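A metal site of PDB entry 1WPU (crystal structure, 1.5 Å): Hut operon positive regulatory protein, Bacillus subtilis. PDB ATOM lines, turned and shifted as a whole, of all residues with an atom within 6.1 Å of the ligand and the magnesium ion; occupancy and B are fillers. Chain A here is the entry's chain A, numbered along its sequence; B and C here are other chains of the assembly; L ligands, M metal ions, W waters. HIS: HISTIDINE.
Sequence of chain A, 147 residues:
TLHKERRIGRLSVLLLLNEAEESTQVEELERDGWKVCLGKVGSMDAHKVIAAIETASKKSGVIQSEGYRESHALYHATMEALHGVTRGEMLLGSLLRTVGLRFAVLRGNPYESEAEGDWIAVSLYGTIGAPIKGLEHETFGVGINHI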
ATOM      1  N   VAL A  85       8.336   9.748 -30.106  1.00  0.00           N
ATOM      2  CA  VAL A  85       9.057   9.805 -28.853  1.00  0.00           C
ATOM      3  C   VAL A  85       9.249   8.433 -28.226  1.00  0.00           C
ATOM      4  O   VAL A  85      10.336   8.111 -27.745  1.00  0.00           O
ATOM      5  CB  VAL A  85       8.341  10.734 -27.847  1.00  0.00           C
ATOM      6  CG1 VAL A  85       8.975  10.601 -26.451  1.00  0.00           C
ATOM      7  CG2 VAL A  85       8.409  12.171 -28.331  1.00  0.00           C
ATOM      8  N   THR A  86       8.193   7.620 -28.227  1.00  0.00           N
ATOM      9  CA  THR A  86       8.241   6.299 -27.605  1.00  0.00           C
ATOM     10  C   THR A  86       8.681   5.147 -28.499  1.00  0.00           C
ATOM     11  O   THR A  86       9.128   4.106 -28.013  1.00  0.00           O
ATOM     12  CB  THR A  86       6.897   5.951 -26.951  1.00  0.00           C
ATOM     13  OG1 THR A  86       5.858   6.011 -27.932  1.00  0.00           O
ATOM     14  CG2 THR A  86       6.574   6.949 -25.832  1.00  0.00           C
ATOM     15  N   ARG A  87       8.529   5.308 -29.815  1.00  0.00           N
ATOM     16  CA  ARG A  87       8.964   4.303 -30.788  1.00  0.00           C
ATOM     17  C   ARG A  87       8.596   2.833 -30.561  1.00  0.00           C
ATOM     18  O   ARG A  87       9.491   1.983 -30.474  1.00  0.00           O
ATOM     19  CB  ARG A  87      10.476   4.427 -30.977  1.00  0.00           C
ATOM     20  CG  ARG A  87      10.919   5.708 -31.667  1.00  0.00           C
ATOM     21  CD  ARG A  87      12.248   6.223 -31.123  1.00  0.00           C
ATOM     22  NE  ARG A  87      12.103   6.568 -29.712  1.00  0.00           N
ATOM     23  CZ  ARG A  87      12.837   6.060 -28.731  1.00  0.00           C
ATOM     24  NH1 ARG A  87      13.804   5.183 -28.992  1.00  0.00           N
ATOM     25  NH2 ARG A  87      12.580   6.388 -27.471  1.00  0.00           N
ATOM     26  N   LEU A  95       8.066   1.120 -18.362  1.00  0.00           N
ATOM     27  CA  LEU A  95       9.198   0.477 -19.028  1.00  0.00           C
ATOM     28  C   LEU A  95      10.505   1.055 -18.511  1.00  0.00           C
ATOM     29  O   LEU A  95      11.528   1.050 -19.190  1.00  0.00           O
ATOM     30  CB  LEU A  95       9.105   0.647 -20.547  1.00  0.00           C
ATOM     31  CG  LEU A  95       7.944  -0.076 -21.232  1.00  0.00           C
ATOM     32  CD1 LEU A  95       8.111   0.075 -22.743  1.00  0.00           C
ATOM     33  CD2 LEU A  95       7.916  -1.543 -20.850  1.00  0.00           C
ATOM     34  N   LEU A  96      10.465   1.560 -17.285  1.00  0.00           N
ATOM     35  CA  LEU A  96      11.624   2.132 -16.615  1.00  0.00           C
ATOM     36  C   LEU A  96      12.337   3.234 -17.380  1.00  0.00           C
ATOM     37  O   LEU A  96      13.558   3.266 -17.471  1.00  0.00           O
ATOM     38  CB  LEU A  96      12.624   1.005 -16.263  1.00  0.00           C
ATOM     39  CG  LEU A  96      13.556   1.302 -15.091  1.00  0.00           C
ATOM     40  CD1 LEU A  96      12.744   1.642 -13.844  1.00  0.00           C
ATOM     41  CD2 LEU A  96      14.449   0.098 -14.833  1.00  0.00           C
ATOM     42  N   ARG A  97      11.557   4.157 -17.951  1.00  0.00           N
ATOM     43  CA  ARG A  97      12.155   5.288 -18.641  1.00  0.00           C
ATOM     44  C   ARG A  97      11.378   6.554 -18.344  1.00  0.00           C
ATOM     45  O   ARG A  97      10.208   6.517 -17.969  1.00  0.00           O
ATOM     46  CB  ARG A  97      12.286   5.034 -20.149  1.00  0.00           C
ATOM     47  CG  ARG A  97      11.004   4.853 -20.906  1.00  0.00           C
ATOM     48  CD  ARG A  97      11.293   4.525 -22.370  1.00  0.00           C
ATOM     49  NE  ARG A  97      10.049   4.253 -23.081  1.00  0.00           N
ATOM     50  CZ  ARG A  97       9.969   3.978 -24.386  1.00  0.00           C
ATOM     51  NH1 ARG A  97      11.057   3.935 -25.143  1.00  0.00           N
ATOM     52  NH2 ARG A  97       8.780   3.713 -24.917  1.00  0.00           N
ATOM     53  N   THR A  98      12.073   7.669 -18.515  1.00  0.00           N
ATOM     54  CA  THR A  98      11.517   8.987 -18.242  1.00  0.00           C
ATOM     55  C   THR A  98      11.831   9.935 -19.389  1.00  0.00           C
ATOM     56  O   THR A  98      12.815   9.735 -20.116  1.00  0.00           O
ATOM     57  CB  THR A  98      12.157   9.531 -16.941  1.00  0.00           C
ATOM     58  OG1 THR A  98      11.801  10.901 -16.745  1.00  0.00           O
ATOM     59  CG2 THR A  98      13.678   9.401 -17.005  1.00  0.00           C
ATOM     60  N   ILE A 128      15.093  11.144 -23.522  1.00  0.00           N
ATOM     61  CA  ILE A 128      14.407   9.989 -22.948  1.00  0.00           C
ATOM     62  C   ILE A 128      15.519   9.079 -22.422  1.00  0.00           C
ATOM     63  O   ILE A 128      16.576   8.992 -23.026  1.00  0.00           O
ATOM     64  CB  ILE A 128      13.529   9.261 -24.018  1.00  0.00           C
ATOM     65  CG1 ILE A 128      12.689   8.184 -23.344  1.00  0.00           C
ATOM     66  CG2 ILE A 128      14.415   8.652 -25.099  1.00  0.00           C
ATOM     67  CD1 ILE A 128      11.573   7.669 -24.251  1.00  0.00           C
ATOM     68  N   GLY A 129      15.284   8.431 -21.290  1.00  0.00           N
ATOM     69  CA  GLY A 129      16.311   7.552 -20.770  1.00  0.00           C
ATOM     70  C   GLY A 129      15.944   6.870 -19.466  1.00  0.00           C
ATOM     71  O   GLY A 129      14.788   6.880 -19.048  1.00  0.00           O
ATOM     72  N   ALA A 130      16.941   6.258 -18.838  1.00  0.00           N
ATOM     73  CA  ALA A 130      16.747   5.593 -17.564  1.00  0.00           C
ATOM     74  C   ALA A 130      16.561   6.695 -16.541  1.00  0.00           C
ATOM     75  O   ALA A 130      16.969   7.846 -16.767  1.00  0.00           O
ATOM     76  CB  ALA A 130      17.970   4.758 -17.232  1.00  0.00           C
ATOM     77  N   PRO A 131      15.949   6.374 -15.391  1.00  0.00           N
ATOM     78  CA  PRO A 131      15.717   7.369 -14.335  1.00  0.00           C
ATOM     79  C   PRO A 131      17.002   7.762 -13.598  1.00  0.00           C
ATOM     80  O   PRO A 131      17.040   7.723 -12.375  1.00  0.00           O
ATOM     81  CB  PRO A 131      14.719   6.666 -13.405  1.00  0.00           C
ATOM     82  CG  PRO A 131      14.099   5.604 -14.265  1.00  0.00           C
ATOM     83  CD  PRO A 131      15.260   5.124 -15.073  1.00  0.00           C
ATOM     84  N   LEU A 135      21.948   9.235 -18.261  1.00  0.00           N
ATOM     85  CA  LEU A 135      21.712   7.979 -18.975  1.00  0.00           C
ATOM     86  C   LEU A 135      20.497   8.208 -19.859  1.00  0.00           C
ATOM     87  O   LEU A 135      19.412   7.676 -19.621  1.00  0.00           O
ATOM     88  CB  LEU A 135      21.433   6.845 -17.985  1.00  0.00           C
ATOM     89  CG  LEU A 135      22.511   6.621 -16.919  1.00  0.00           C
ATOM     90  CD1 LEU A 135      22.185   5.342 -16.146  1.00  0.00           C
ATOM     91  CD2 LEU A 135      23.889   6.510 -17.549  1.00  0.00           C
ATOM     92  N   GLU A 136      20.704   9.002 -20.905  1.00  0.00           N
ATOM     93  CA  GLU A 136      19.613   9.372 -21.792  1.00  0.00           C
ATOM     94  C   GLU A 136      20.140   9.821 -23.157  1.00  0.00           C
ATOM     95  O   GLU A 136      21.330  10.083 -23.329  1.00  0.00           O
ATOM     96  CB  GLU A 136      18.868  10.552 -21.151  1.00  0.00           C
ATOM     97  CG  GLU A 136      19.712  11.840 -21.101  1.00  0.00           C
ATOM     98  CD  GLU A 136      19.397  12.744 -19.917  1.00  0.00           C
ATOM     99  OE1 GLU A 136      19.492  13.981 -20.070  1.00  0.00           O
ATOM    100  OE2 GLU A 136      19.092  12.240 -18.817  1.00  0.00           O
ATOM    101  N   HIS A 137      19.230   9.874 -24.124  1.00  0.00           N
ATOM    102  CA  HIS A 137      19.552  10.381 -25.451  1.00  0.00           C
ATOM    103  C   HIS A 137      18.360  11.194 -25.929  1.00  0.00           C
ATOM    104  O   HIS A 137      17.305  11.208 -25.286  1.00  0.00           O
ATOM    105  CB  HIS A 137      19.964   9.268 -26.451  1.00  0.00           C
ATOM    106  CG  HIS A 137      18.930   8.223 -26.702  1.00  0.00           C
ATOM    107  ND1 HIS A 137      17.715   8.506 -27.310  1.00  0.00           N
ATOM    108  CD2 HIS A 137      18.950   6.887 -26.514  1.00  0.00           C
ATOM    109  CE1 HIS A 137      17.042   7.381 -27.476  1.00  0.00           C
ATOM    110  NE2 HIS A 137      17.773   6.386 -26.996  1.00  0.00           N
ATOM    111  N   TYR B  68      26.660   5.398 -20.242  1.00  0.00           N
ATOM    112  CA  TYR B  68      25.345   5.069 -20.801  1.00  0.00           C
ATOM    113  C   TYR B  68      25.379   3.998 -21.887  1.00  0.00           C
ATOM    114  O   TYR B  68      24.494   3.145 -21.934  1.00  0.00           O
ATOM    115  CB  TYR B  68      24.696   6.335 -21.372  1.00  0.00           C
ATOM    116  CG  TYR B  68      23.285   6.156 -21.883  1.00  0.00           C
ATOM    117  CD1 TYR B  68      22.344   5.445 -21.132  1.00  0.00           C
ATOM    118  CD2 TYR B  68      22.870   6.741 -23.081  1.00  0.00           C
ATOM    119  CE1 TYR B  68      21.023   5.327 -21.558  1.00  0.00           C
ATOM    120  CE2 TYR B  68      21.545   6.636 -23.509  1.00  0.00           C
ATOM    121  CZ  TYR B  68      20.635   5.923 -22.745  1.00  0.00           C
ATOM    122  OH  TYR B  68      19.320   5.831 -23.145  1.00  0.00           O
ATOM    123  N   SER B  71      24.563   0.412 -20.981  1.00  0.00           N
ATOM    124  CA  SER B  71      23.243   0.327 -20.380  1.00  0.00           C
ATOM    125  C   SER B  71      22.211   0.483 -21.498  1.00  0.00           C
ATOM    126  O   SER B  71      21.156  -0.153 -21.470  1.00  0.00           O
ATOM    127  CB  SER B  71      23.044   1.449 -19.353  1.00  0.00           C
ATOM    128  OG  SER B  71      23.850   1.234 -18.210  1.00  0.00           O
ATOM    129  N   HIS B  72      22.534   1.310 -22.479  1.00  0.00           N
ATOM    130  CA  HIS B  72      21.651   1.531 -23.620  1.00  0.00           C
ATOM    131  C   HIS B  72      21.499   0.228 -24.408  1.00  0.00           C
ATOM    132  O   HIS B  72      20.387  -0.159 -24.778  1.00  0.00           O
ATOM    133  CB  HIS B  72      22.217   2.611 -24.538  1.00  0.00           C
ATOM    134  CG  HIS B  72      21.289   2.988 -25.649  1.00  0.00           C
ATOM    135  ND1 HIS B  72      21.439   2.536 -26.951  1.00  0.00           N
ATOM    136  CD2 HIS B  72      20.159   3.737 -25.651  1.00  0.00           C
ATOM    137  CE1 HIS B  72      20.451   2.995 -27.695  1.00  0.00           C
ATOM    138  NE2 HIS B  72      19.655   3.723 -26.926  1.00  0.00           N
ATOM    139  N   TYR B  75      19.394  -2.238 -22.348  1.00  0.00           N
ATOM    140  CA  TYR B  75      17.984  -1.880 -22.289  1.00  0.00           C
ATOM    141  C   TYR B  75      17.240  -2.337 -23.538  1.00  0.00           C
ATOM    142  O   TYR B  75      16.175  -2.944 -23.456  1.00  0.00           O
ATOM    143  CB  TYR B  75      17.820  -0.371 -22.099  1.00  0.00           C
ATOM    144  CG  TYR B  75      16.379   0.077 -22.014  1.00  0.00           C
ATOM    145  CD1 TYR B  75      15.691   0.521 -23.140  1.00  0.00           C
ATOM    146  CD2 TYR B  75      15.691   0.024 -20.803  1.00  0.00           C
ATOM    147  CE1 TYR B  75      14.346   0.906 -23.061  1.00  0.00           C
ATOM    148  CE2 TYR B  75      14.358   0.394 -20.708  1.00  0.00           C
ATOM    149  CZ  TYR B  75      13.693   0.836 -21.842  1.00  0.00           C
ATOM    150  OH  TYR B  75      12.381   1.231 -21.742  1.00  0.00           O
ATOM    151  N   HIS B  76      17.801  -2.059 -24.703  1.00  0.00           N
ATOM    152  CA  HIS B  76      17.131  -2.449 -25.941  1.00  0.00           C
ATOM    153  C   HIS B  76      17.103  -3.962 -26.138  1.00  0.00           C
ATOM    154  O   HIS B  76      16.133  -4.481 -26.679  1.00  0.00           O
ATOM    155  CB  HIS B  76      17.772  -1.722 -27.107  1.00  0.00           C
ATOM    156  CG  HIS B  76      17.325  -0.294 -27.202  1.00  0.00           C
ATOM    157  ND1 HIS B  76      16.079   0.058 -27.665  1.00  0.00           N
ATOM    158  CD2 HIS B  76      17.930   0.851 -26.830  1.00  0.00           C
ATOM    159  CE1 HIS B  76      15.930   1.369 -27.569  1.00  0.00           C
ATOM    160  NE2 HIS B  76      17.038   1.877 -27.064  1.00  0.00           N
ATOM    161  N   GLU C  80      13.734   3.061 -35.745  1.00  0.00           N
ATOM    162  CA  GLU C  80      13.222   4.005 -34.765  1.00  0.00           C
ATOM    163  C   GLU C  80      12.738   5.293 -35.429  1.00  0.00           C
ATOM    164  O   GLU C  80      11.710   5.836 -35.049  1.00  0.00           O
ATOM    165  CB  GLU C  80      14.290   4.300 -33.704  1.00  0.00           C
ATOM    166  CG  GLU C  80      14.488   3.144 -32.726  1.00  0.00           C
ATOM    167  CD  GLU C  80      15.293   3.528 -31.505  1.00  0.00           C
ATOM    168  OE1 GLU C  80      15.567   4.734 -31.344  1.00  0.00           O
ATOM    169  N   TRP C 119      27.818   7.465 -31.674  1.00  0.00           N
ATOM    170  CA  TRP C 119      26.384   7.229 -31.729  1.00  0.00           C
ATOM    171  C   TRP C 119      25.948   7.638 -33.112  1.00  0.00           C
ATOM    172  O   TRP C 119      26.684   8.314 -33.832  1.00  0.00           O
ATOM    173  CB  TRP C 119      25.659   8.069 -30.670  1.00  0.00           C
ATOM    174  CG  TRP C 119      25.916   7.568 -29.291  1.00  0.00           C
ATOM    175  CD1 TRP C 119      27.105   7.561 -28.630  1.00  0.00           C
ATOM    176  CD2 TRP C 119      24.974   6.927 -28.424  1.00  0.00           C
ATOM    177  NE1 TRP C 119      26.965   6.962 -27.408  1.00  0.00           N
ATOM    178  CE2 TRP C 119      25.666   6.559 -27.254  1.00  0.00           C
ATOM    179  CE3 TRP C 119      23.608   6.623 -28.527  1.00  0.00           C
ATOM    180  CZ2 TRP C 119      25.051   5.914 -26.179  1.00  0.00           C
ATOM    181  CZ3 TRP C 119      22.993   5.976 -27.462  1.00  0.00           C
ATOM    182  CH2 TRP C 119      23.718   5.622 -26.303  1.00  0.00           C
ATOM    183  N   ILE C 144      17.885   7.231 -32.750  1.00  0.00           N
ATOM    184  CA  ILE C 144      19.241   7.375 -32.214  1.00  0.00           C
ATOM    185  C   ILE C 144      19.716   6.026 -31.649  1.00  0.00           C
ATOM    186  O   ILE C 144      18.963   5.338 -30.980  1.00  0.00           O
ATOM    187  CB  ILE C 144      19.272   8.451 -31.102  1.00  0.00           C
ATOM    188  CG1 ILE C 144      18.981   9.831 -31.720  1.00  0.00           C
ATOM    189  CG2 ILE C 144      20.636   8.474 -30.401  1.00  0.00           C
ATOM    190  CD1 ILE C 144      18.883  10.962 -30.727  1.00  0.00           C
ATOM    191  N   ASN C 145      20.967   5.661 -31.928  1.00  0.00           N
ATOM    192  CA  ASN C 145      21.499   4.391 -31.450  1.00  0.00           C
ATOM    193  C   ASN C 145      22.994   4.506 -31.215  1.00  0.00           C
ATOM    194  O   ASN C 145      23.641   5.419 -31.722  1.00  0.00           O
ATOM    195  CB  ASN C 145      21.211   3.302 -32.500  1.00  0.00           C
ATOM    196  CG  ASN C 145      21.199   1.914 -31.909  1.00  0.00           C
ATOM    197  OD1 ASN C 145      21.202   1.732 -30.684  1.00  0.00           O
ATOM    198  ND2 ASN C 145      21.167   0.901 -32.768  1.00  0.00           N
HETATM  199  CA  HIS L   1      15.724   4.070 -24.378  1.00  0.00           C
HETATM  200  C   HIS L   1      14.846   4.589 -25.510  1.00  0.00           C
HETATM  201  O   HIS L   1      15.310   4.599 -26.659  1.00  0.00           O
HETATM  202  CB  HIS L   1      15.491   4.859 -23.096  1.00  0.00           C
HETATM  203  CG  HIS L   1      16.190   4.251 -21.907  1.00  0.00           C
HETATM  204  ND1 HIS L   1      17.556   4.264 -21.773  1.00  0.00           N
HETATM  205  CD2 HIS L   1      15.703   3.533 -20.864  1.00  0.00           C
HETATM  206  CE1 HIS L   1      17.889   3.571 -20.701  1.00  0.00           C
HETATM  207  NE2 HIS L   1      16.782   3.116 -20.133  1.00  0.00           N
HETATM  208  OXT HIS L   1      13.696   4.967 -25.245  1.00  0.00           O
HETATM  209 MG    MG M   1      17.389   4.145 -27.004  1.00  0.00          MG
HETATM  210  O   HOH W   1      17.276   4.127 -29.172  1.00  0.00           O
HETATM  211  O   HOH W   2      16.036   2.081 -17.567  1.00  0.00           O
HETATM  212  O   HOH W   3      19.434   1.661 -18.252  1.00  0.00           O
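The backbone NH (N) of Ile 128 lies within hydrogen-bond range of the backbone carbonyl oxygen (O) of His 137, 2.8 Å away. NH2 of Arg 97 is in hydrogen-bond range of O of Thr 86, 3.1 Å away. NH1 of Arg 87 is in salt-bridge range of OE1 of Glu 80 of chain C, 3.0 Å away. The guanidinium group (NH2) of Arg 87 is in hydrogen-bond range of the backbone carbonyl oxygen (O) of Val 85, 2.8 Å away. The side-chain hydroxyl (OH) of Tyr 75 of chain B is in hydrogen-bond range of the backbone carbonyl oxygen (O) of Leu 95 (2.7 Å). The backbone NH (N) of Ala 130 sits at hydrogen-bond distance from the backbone carbonyl oxygen (O) of Leu 135. The backbone NH (N) of Thr 98 lies within hydrogen-bond range of the backbone carbonyl oxygen (O) of Gly 129 (2.9 Å).
O of the ligand binds the magnesium ion, 2.2 Å away. Water W1 binds the magnesium ion, 2.2 Å away. NE2 of His 137 is bound to the magnesium ion (2.3 Å). A ring nitrogen (NE2) of His 76 of chain B is bound to the magnesium ion, 2.3 Å away. The magnesium ion is bound by NE2 of His 72 of chain B (2.3 Å). The magnesium ion has five donor atoms within binding distance.
ND1 of the ligand sits at hydrogen-bond distance from OH of Tyr 68 of chain B (2.7 Å). NH1 of Arg 97 lies within salt-bridge range of OXT of the ligand, 2.8 Å away. An oxygen (OXT) of the ligand is in salt-bridge range of the guanidinium group of Arg 87. The backbone NH (N) of Ala 130 sits close to a nitrogen (NE2) of the ligand, 3.4 Å away.
Residues that only touch the ligand: Ile 128 (3.6 Å), Gly 129 (3.5 Å) and Tyr 75 of chain B (3.3 Å). Within 4 Å of the ligand: Arg 87, Arg 97, Ile 128, Gly 129, Ala 130, His 137, Tyr 68 of chain B, Tyr 75 of chain B and His 76 of chain B. The nearest printed residue that does not touch the ligand is Leu 96 (4.02 Å).
Water W1 bridges O of Ile 144 of chain C (2.8 Å) and OE1 of Glu 80 of chain C (2.8 Å). Water W2 lies within hydrogen-bond range of the backbone carbonyl oxygen of Leu 96 (2.7 Å) and a nitrogen (NE2) of the ligand (2.9 Å).
Within 4 Å of the magnesium ion: His 137, His 72 of chain B and His 76 of chain B. The nearest printed residue that does not touch the magnesium ion is Arg 87 (4.2 Å).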
